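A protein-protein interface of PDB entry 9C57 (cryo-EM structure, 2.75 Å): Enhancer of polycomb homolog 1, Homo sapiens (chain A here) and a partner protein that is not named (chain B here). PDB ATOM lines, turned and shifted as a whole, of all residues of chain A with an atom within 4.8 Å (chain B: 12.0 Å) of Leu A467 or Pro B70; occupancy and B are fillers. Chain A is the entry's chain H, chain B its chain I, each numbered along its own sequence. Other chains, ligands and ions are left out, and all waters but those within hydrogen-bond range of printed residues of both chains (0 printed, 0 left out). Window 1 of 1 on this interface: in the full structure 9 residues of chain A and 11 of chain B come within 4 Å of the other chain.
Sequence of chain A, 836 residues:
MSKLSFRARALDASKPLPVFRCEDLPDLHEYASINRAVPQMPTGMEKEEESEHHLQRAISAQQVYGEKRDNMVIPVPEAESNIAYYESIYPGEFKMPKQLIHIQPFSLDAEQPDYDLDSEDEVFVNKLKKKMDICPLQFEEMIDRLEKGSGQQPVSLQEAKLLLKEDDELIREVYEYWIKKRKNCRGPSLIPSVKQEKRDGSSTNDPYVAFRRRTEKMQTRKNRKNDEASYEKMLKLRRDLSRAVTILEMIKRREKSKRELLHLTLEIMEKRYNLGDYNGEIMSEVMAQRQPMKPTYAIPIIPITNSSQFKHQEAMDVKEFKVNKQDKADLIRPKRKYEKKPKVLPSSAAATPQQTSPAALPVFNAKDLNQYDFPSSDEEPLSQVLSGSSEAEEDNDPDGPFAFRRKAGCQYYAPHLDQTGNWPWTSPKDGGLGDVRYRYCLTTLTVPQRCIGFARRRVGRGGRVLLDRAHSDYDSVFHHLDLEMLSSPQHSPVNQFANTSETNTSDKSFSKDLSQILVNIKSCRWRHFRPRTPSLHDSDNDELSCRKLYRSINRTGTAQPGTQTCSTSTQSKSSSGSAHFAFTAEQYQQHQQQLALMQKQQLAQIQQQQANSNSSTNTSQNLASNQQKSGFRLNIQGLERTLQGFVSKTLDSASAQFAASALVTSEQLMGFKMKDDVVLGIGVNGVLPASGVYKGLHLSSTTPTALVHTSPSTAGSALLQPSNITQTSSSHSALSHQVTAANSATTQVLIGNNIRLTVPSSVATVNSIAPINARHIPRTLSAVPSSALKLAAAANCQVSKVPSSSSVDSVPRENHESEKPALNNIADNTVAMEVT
The backbone NH of Leu B71 sits at hydrogen-bond distance from the backbone carbonyl oxygen of Leu A467.
The guanidinium group (NH2) of Arg A469 is in hydrogen-bond range of the backbone carbonyl oxygen (O) of Pro B69 (2.4 Å).
The side-chain amino group of Lys B65 is in salt-bridge range of the side-chain carboxylate of Asp B67 (3.5 Å).
Pro B73 touches Val A465.
Leu A466 touches Leu B71.
CD2 of Leu A466 touches CG of Leu B72 (3.8 Å).
CD2 of Leu A466 touches CD of Pro B73, at 3.3 Å.
Pro B70 touches Leu A467.
Lys B65 touches Arg A469.
CB of Asp B67 touches O of Arg A469, at 3.4 Å.
Ala B68 touches Arg A469.
Leu B71 touches Arg A469 (CD1 to CZ, 3.2 Å).
No residue of chain B comes within 4 Å of Arg A457.
Of chain B, only Pro B73 comes within 4 Å of Val A465.
Of the printed residues of chain B, Leu A467 touches Pro B70 (3.5 Å) and Leu B71 (2.7 Å).
No residue of chain B comes within 4 Å of Asp A468.
Asp B64 touches none of the printed residues of chain A.
Printed residues of chain A within 4 Å of Lys B65: Arg A469.
Of the printed residues of chain A, Pro B70 touches Leu A467 (3.5 Å).
Of the printed residues of chain A, Leu B72 touches Leu A466 (3.8 Å).
Ser B74 touches none of the printed residues of chain A.
The nearest residue of chain A that does not touch Pro B70 is Arg A469 (4.3 Å).
The nearest printed residue of chain A that does not touch Lys B65 is Asp A468 (5.7 Å).
Of the 8 printed residues of chain A, 4 touch a printed residue of chain B.
Of the 12 printed residues of chain B, 8 touch a printed residue of chain A.
Among the printed residues, no Asp or Glu carboxylate lies within 4 Å of a Lys or Arg side-chain nitrogen of the other chain.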
ATOM      1  N   ALA A 455      -6.928  17.917   3.147  1.00  0.00           N
ATOM      2  CA  ALA A 455      -7.375  19.146   2.515  1.00  0.00           C
ATOM      3  C   ALA A 455      -7.833  20.110   3.598  1.00  0.00           C
ATOM      4  O   ALA A 455      -8.441  19.703   4.590  1.00  0.00           O
ATOM      5  CB  ALA A 455      -8.509  18.885   1.518  1.00  0.00           C
ATOM      6  N   ARG A 456      -7.535  21.392   3.399  1.00  0.00           N
ATOM      7  CA  ARG A 456      -7.933  22.433   4.335  1.00  0.00           C
ATOM      8  C   ARG A 456      -8.592  23.571   3.571  1.00  0.00           C
ATOM      9  O   ARG A 456      -8.329  23.780   2.384  1.00  0.00           O
ATOM     10  CB  ARG A 456      -6.739  22.958   5.141  1.00  0.00           C
ATOM     11  CG  ARG A 456      -5.604  23.507   4.304  1.00  0.00           C
ATOM     12  CD  ARG A 456      -5.657  25.019   4.237  1.00  0.00           C
ATOM     13  NE  ARG A 456      -4.490  25.567   3.558  1.00  0.00           N
ATOM     14  CZ  ARG A 456      -3.364  25.918   4.163  1.00  0.00           C
ATOM     15  NH1 ARG A 456      -3.206  25.779   5.469  1.00  0.00           N
ATOM     16  NH2 ARG A 456      -2.367  26.415   3.437  1.00  0.00           N
ATOM     17  N   ARG A 457      -9.450  24.307   4.265  1.00  0.00           N
ATOM     18  CA  ARG A 457     -10.317  25.288   3.634  1.00  0.00           C
ATOM     19  C   ARG A 457      -9.716  26.681   3.761  1.00  0.00           C
ATOM     20  O   ARG A 457      -9.060  27.009   4.750  1.00  0.00           O
ATOM     21  CB  ARG A 457     -11.715  25.268   4.254  1.00  0.00           C
ATOM     22  CG  ARG A 457     -12.154  23.908   4.777  1.00  0.00           C
ATOM     23  CD  ARG A 457     -13.343  24.039   5.704  1.00  0.00           C
ATOM     24  NE  ARG A 457     -14.620  23.985   5.005  1.00  0.00           N
ATOM     25  CZ  ARG A 457     -15.278  25.041   4.551  1.00  0.00           C
ATOM     26  NH1 ARG A 457     -14.746  26.250   4.574  1.00  0.00           N
ATOM     27  NH2 ARG A 457     -16.496  24.875   4.042  1.00  0.00           N
ATOM     28  N   VAL A 465     -14.587  30.061  -1.216  1.00  0.00           N
ATOM     29  CA  VAL A 465     -14.013  29.102  -0.281  1.00  0.00           C
ATOM     30  C   VAL A 465     -13.370  27.970  -1.073  1.00  0.00           C
ATOM     31  O   VAL A 465     -14.051  27.229  -1.789  1.00  0.00           O
ATOM     32  CB  VAL A 465     -15.078  28.575   0.693  1.00  0.00           C
ATOM     33  CG1 VAL A 465     -16.126  27.769  -0.042  1.00  0.00           C
ATOM     34  CG2 VAL A 465     -14.438  27.737   1.778  1.00  0.00           C
ATOM     35  N   LEU A 466     -12.056  27.835  -0.940  1.00  0.00           N
ATOM     36  CA  LEU A 466     -11.281  26.867  -1.695  1.00  0.00           C
ATOM     37  C   LEU A 466     -10.728  25.802  -0.760  1.00  0.00           C
ATOM     38  O   LEU A 466     -10.320  26.094   0.368  1.00  0.00           O
ATOM     39  CB  LEU A 466     -10.119  27.541  -2.440  1.00  0.00           C
ATOM     40  CG  LEU A 466     -10.346  28.972  -2.932  1.00  0.00           C
ATOM     41  CD1 LEU A 466      -9.099  29.516  -3.603  1.00  0.00           C
ATOM     42  CD2 LEU A 466     -11.521  29.039  -3.882  1.00  0.00           C
ATOM     43  N   LEU A 467     -10.717  24.565  -1.239  1.00  0.00           N
ATOM     44  CA  LEU A 467     -10.060  23.464  -0.552  1.00  0.00           C
ATOM     45  C   LEU A 467      -8.672  23.256  -1.141  1.00  0.00           C
ATOM     46  O   LEU A 467      -8.532  22.991  -2.339  1.00  0.00           O
ATOM     47  CB  LEU A 467     -10.873  22.173  -0.664  1.00  0.00           C
ATOM     48  CG  LEU A 467     -12.033  21.922   0.304  1.00  0.00           C
ATOM     49  CD1 LEU A 467     -11.559  22.001   1.746  1.00  0.00           C
ATOM     50  CD2 LEU A 467     -13.191  22.868   0.071  1.00  0.00           C
ATOM     51  N   ASP A 468      -7.655  23.384  -0.299  1.00  0.00           N
ATOM     52  CA  ASP A 468      -6.287  23.034  -0.646  1.00  0.00           C
ATOM     53  C   ASP A 468      -6.110  21.531  -0.476  1.00  0.00           C
ATOM     54  O   ASP A 468      -6.995  20.839   0.029  1.00  0.00           O
ATOM     55  CB  ASP A 468      -5.300  23.792   0.237  1.00  0.00           C
ATOM     56  CG  ASP A 468      -4.136  24.345  -0.539  1.00  0.00           C
ATOM     57  OD1 ASP A 468      -3.324  23.548  -1.050  1.00  0.00           O
ATOM     58  OD2 ASP A 468      -4.041  25.584  -0.637  1.00  0.00           O
ATOM     59  N   ARG A 469      -4.957  21.019  -0.902  1.00  0.00           N
ATOM     60  CA  ARG A 469      -4.738  19.582  -0.846  1.00  0.00           C
ATOM     61  C   ARG A 469      -3.267  19.245  -0.666  1.00  0.00           C
ATOM     62  O   ARG A 469      -2.379  20.052  -0.953  1.00  0.00           O
ATOM     63  CB  ARG A 469      -5.263  18.892  -2.105  1.00  0.00           C
ATOM     64  CG  ARG A 469      -6.769  18.914  -2.228  1.00  0.00           C
ATOM     65  CD  ARG A 469      -7.213  18.156  -3.451  1.00  0.00           C
ATOM     66  NE  ARG A 469      -6.784  18.828  -4.670  1.00  0.00           N
ATOM     67  CZ  ARG A 469      -6.974  18.353  -5.890  1.00  0.00           C
ATOM     68  NH1 ARG A 469      -7.596  17.206  -6.098  1.00  0.00           N
ATOM     69  NH2 ARG A 469      -6.534  19.052  -6.930  1.00  0.00           N
ATOM     70  N   SER B  63       2.627  27.984   2.087  1.00  0.00           N
ATOM     71  CA  SER B  63       2.190  27.970   0.662  1.00  0.00           C
ATOM     72  C   SER B  63       1.734  26.583   0.236  1.00  0.00           C
ATOM     73  O   SER B  63       0.540  26.316   0.126  1.00  0.00           O
ATOM     74  CB  SER B  63       3.319  28.442  -0.254  1.00  0.00           C
ATOM     75  OG  SER B  63       3.596  29.816  -0.061  1.00  0.00           O
ATOM     76  N   ASP B  64       2.695  25.700   0.001  1.00  0.00           N
ATOM     77  CA  ASP B  64       2.410  24.363  -0.502  1.00  0.00           C
ATOM     78  C   ASP B  64       3.672  23.524  -0.346  1.00  0.00           C
ATOM     79  O   ASP B  64       4.725  24.017   0.072  1.00  0.00           O
ATOM     80  CB  ASP B  64       1.957  24.408  -1.962  1.00  0.00           C
ATOM     81  CG  ASP B  64       2.934  25.155  -2.849  1.00  0.00           C
ATOM     82  OD1 ASP B  64       4.093  24.707  -2.976  1.00  0.00           O
ATOM     83  OD2 ASP B  64       2.549  26.196  -3.416  1.00  0.00           O
ATOM     84  N   LYS B  65       3.550  22.245  -0.681  1.00  0.00           N
ATOM     85  CA  LYS B  65       4.681  21.329  -0.788  1.00  0.00           C
ATOM     86  C   LYS B  65       4.533  20.461  -2.036  1.00  0.00           C
ATOM     87  O   LYS B  65       4.691  19.241  -2.003  1.00  0.00           O
ATOM     88  CB  LYS B  65       4.858  20.510   0.495  1.00  0.00           C
ATOM     89  CG  LYS B  65       3.800  19.452   0.791  1.00  0.00           C
ATOM     90  CD  LYS B  65       2.521  20.129   1.263  1.00  0.00           C
ATOM     91  CE  LYS B  65       1.417  19.155   1.606  1.00  0.00           C
ATOM     92  NZ  LYS B  65       0.093  19.836   1.516  1.00  0.00           N
ATOM     93  N   LYS B  66       4.240  21.106  -3.167  1.00  0.00           N
ATOM     94  CA  LYS B  66       4.209  20.451  -4.475  1.00  0.00           C
ATOM     95  C   LYS B  66       3.178  19.316  -4.486  1.00  0.00           C
ATOM     96  O   LYS B  66       3.505  18.131  -4.556  1.00  0.00           O
ATOM     97  CB  LYS B  66       5.607  19.942  -4.847  1.00  0.00           C
ATOM     98  CG  LYS B  66       5.836  19.741  -6.344  1.00  0.00           C
ATOM     99  CD  LYS B  66       5.112  18.519  -6.915  1.00  0.00           C
ATOM    100  CE  LYS B  66       5.561  17.200  -6.286  1.00  0.00           C
ATOM    101  NZ  LYS B  66       4.634  16.080  -6.613  1.00  0.00           N
ATOM    102  N   ASP B  67       1.916  19.716  -4.392  1.00  0.00           N
ATOM    103  CA  ASP B  67       0.805  18.785  -4.247  1.00  0.00           C
ATOM    104  C   ASP B  67      -0.251  19.049  -5.316  1.00  0.00           C
ATOM    105  O   ASP B  67      -0.041  19.817  -6.258  1.00  0.00           O
ATOM    106  CB  ASP B  67       0.210  18.905  -2.847  1.00  0.00           C
ATOM    107  CG  ASP B  67       1.269  18.933  -1.775  1.00  0.00           C
ATOM    108  OD1 ASP B  67       1.793  20.030  -1.505  1.00  0.00           O
ATOM    109  OD2 ASP B  67       1.602  17.860  -1.231  1.00  0.00           O
ATOM    110  N   ALA B  68      -1.405  18.406  -5.152  1.00  0.00           N
ATOM    111  CA  ALA B  68      -2.495  18.558  -6.096  1.00  0.00           C
ATOM    112  C   ALA B  68      -2.994  20.001  -6.098  1.00  0.00           C
ATOM    113  O   ALA B  68      -2.875  20.711  -5.097  1.00  0.00           O
ATOM    114  CB  ALA B  68      -3.633  17.605  -5.740  1.00  0.00           C
ATOM    115  N   PRO B  69      -3.561  20.456  -7.211  1.00  0.00           N
ATOM    116  CA  PRO B  69      -3.986  21.853  -7.309  1.00  0.00           C
ATOM    117  C   PRO B  69      -5.153  22.130  -6.381  1.00  0.00           C
ATOM    118  O   PRO B  69      -5.864  21.199  -5.972  1.00  0.00           O
ATOM    119  CB  PRO B  69      -4.397  21.989  -8.781  1.00  0.00           C
ATOM    120  CG  PRO B  69      -4.847  20.631  -9.146  1.00  0.00           C
ATOM    121  CD  PRO B  69      -3.905  19.704  -8.431  1.00  0.00           C
ATOM    122  N   PRO B  70      -5.385  23.391  -6.021  1.00  0.00           N
ATOM    123  CA  PRO B  70      -6.530  23.708  -5.164  1.00  0.00           C
ATOM    124  C   PRO B  70      -7.842  23.303  -5.809  1.00  0.00           C
ATOM    125  O   PRO B  70      -7.946  23.115  -7.022  1.00  0.00           O
ATOM    126  CB  PRO B  70      -6.449  25.229  -4.998  1.00  0.00           C
ATOM    127  CG  PRO B  70      -5.079  25.582  -5.323  1.00  0.00           C
ATOM    128  CD  PRO B  70      -4.567  24.580  -6.303  1.00  0.00           C
ATOM    129  N   LEU B  71      -8.857  23.163  -4.969  1.00  0.00           N
ATOM    130  CA  LEU B  71     -10.210  22.894  -5.422  1.00  0.00           C
ATOM    131  C   LEU B  71     -11.037  24.161  -5.235  1.00  0.00           C
ATOM    132  O   LEU B  71     -11.033  24.754  -4.152  1.00  0.00           O
ATOM    133  CB  LEU B  71     -10.810  21.717  -4.651  1.00  0.00           C
ATOM    134  CG  LEU B  71     -11.058  20.416  -5.420  1.00  0.00           C
ATOM    135  CD1 LEU B  71      -9.787  19.846  -5.973  1.00  0.00           C
ATOM    136  CD2 LEU B  71     -11.708  19.405  -4.509  1.00  0.00           C
ATOM    137  N   LEU B  72     -11.728  24.581  -6.294  1.00  0.00           N
ATOM    138  CA  LEU B  72     -12.425  25.859  -6.321  1.00  0.00           C
ATOM    139  C   LEU B  72     -13.938  25.662  -6.364  1.00  0.00           C
ATOM    140  O   LEU B  72     -14.420  24.643  -6.865  1.00  0.00           O
ATOM    141  CB  LEU B  72     -12.002  26.688  -7.540  1.00  0.00           C
ATOM    142  CG  LEU B  72     -10.886  27.708  -7.331  1.00  0.00           C
ATOM    143  CD1 LEU B  72      -9.637  27.038  -6.789  1.00  0.00           C
ATOM    144  CD2 LEU B  72     -10.584  28.429  -8.626  1.00  0.00           C
ATOM    145  N   PRO B  73     -14.711  26.612  -5.843  1.00  0.00           N
ATOM    146  CA  PRO B  73     -16.165  26.555  -6.024  1.00  0.00           C
ATOM    147  C   PRO B  73     -16.553  26.714  -7.484  1.00  0.00           C
ATOM    148  O   PRO B  73     -15.931  27.462  -8.240  1.00  0.00           O
ATOM    149  CB  PRO B  73     -16.680  27.733  -5.189  1.00  0.00           C
ATOM    150  CG  PRO B  73     -15.593  28.053  -4.251  1.00  0.00           C
ATOM    151  CD  PRO B  73     -14.319  27.718  -4.955  1.00  0.00           C
ATOM    152  N   SER B  74     -17.604  25.999  -7.875  1.00  0.00           N
ATOM    153  CA  SER B  74     -18.140  26.130  -9.218  1.00  0.00           C
ATOM    154  C   SER B  74     -19.636  25.871  -9.188  1.00  0.00           C
ATOM    155  O   SER B  74     -20.140  25.094  -8.374  1.00  0.00           O
ATOM    156  CB  SER B  74     -17.464  25.169 -10.197  1.00  0.00           C
ATOM    157  OG  SER B  74     -18.164  23.940 -10.258  1.00  0.00           O
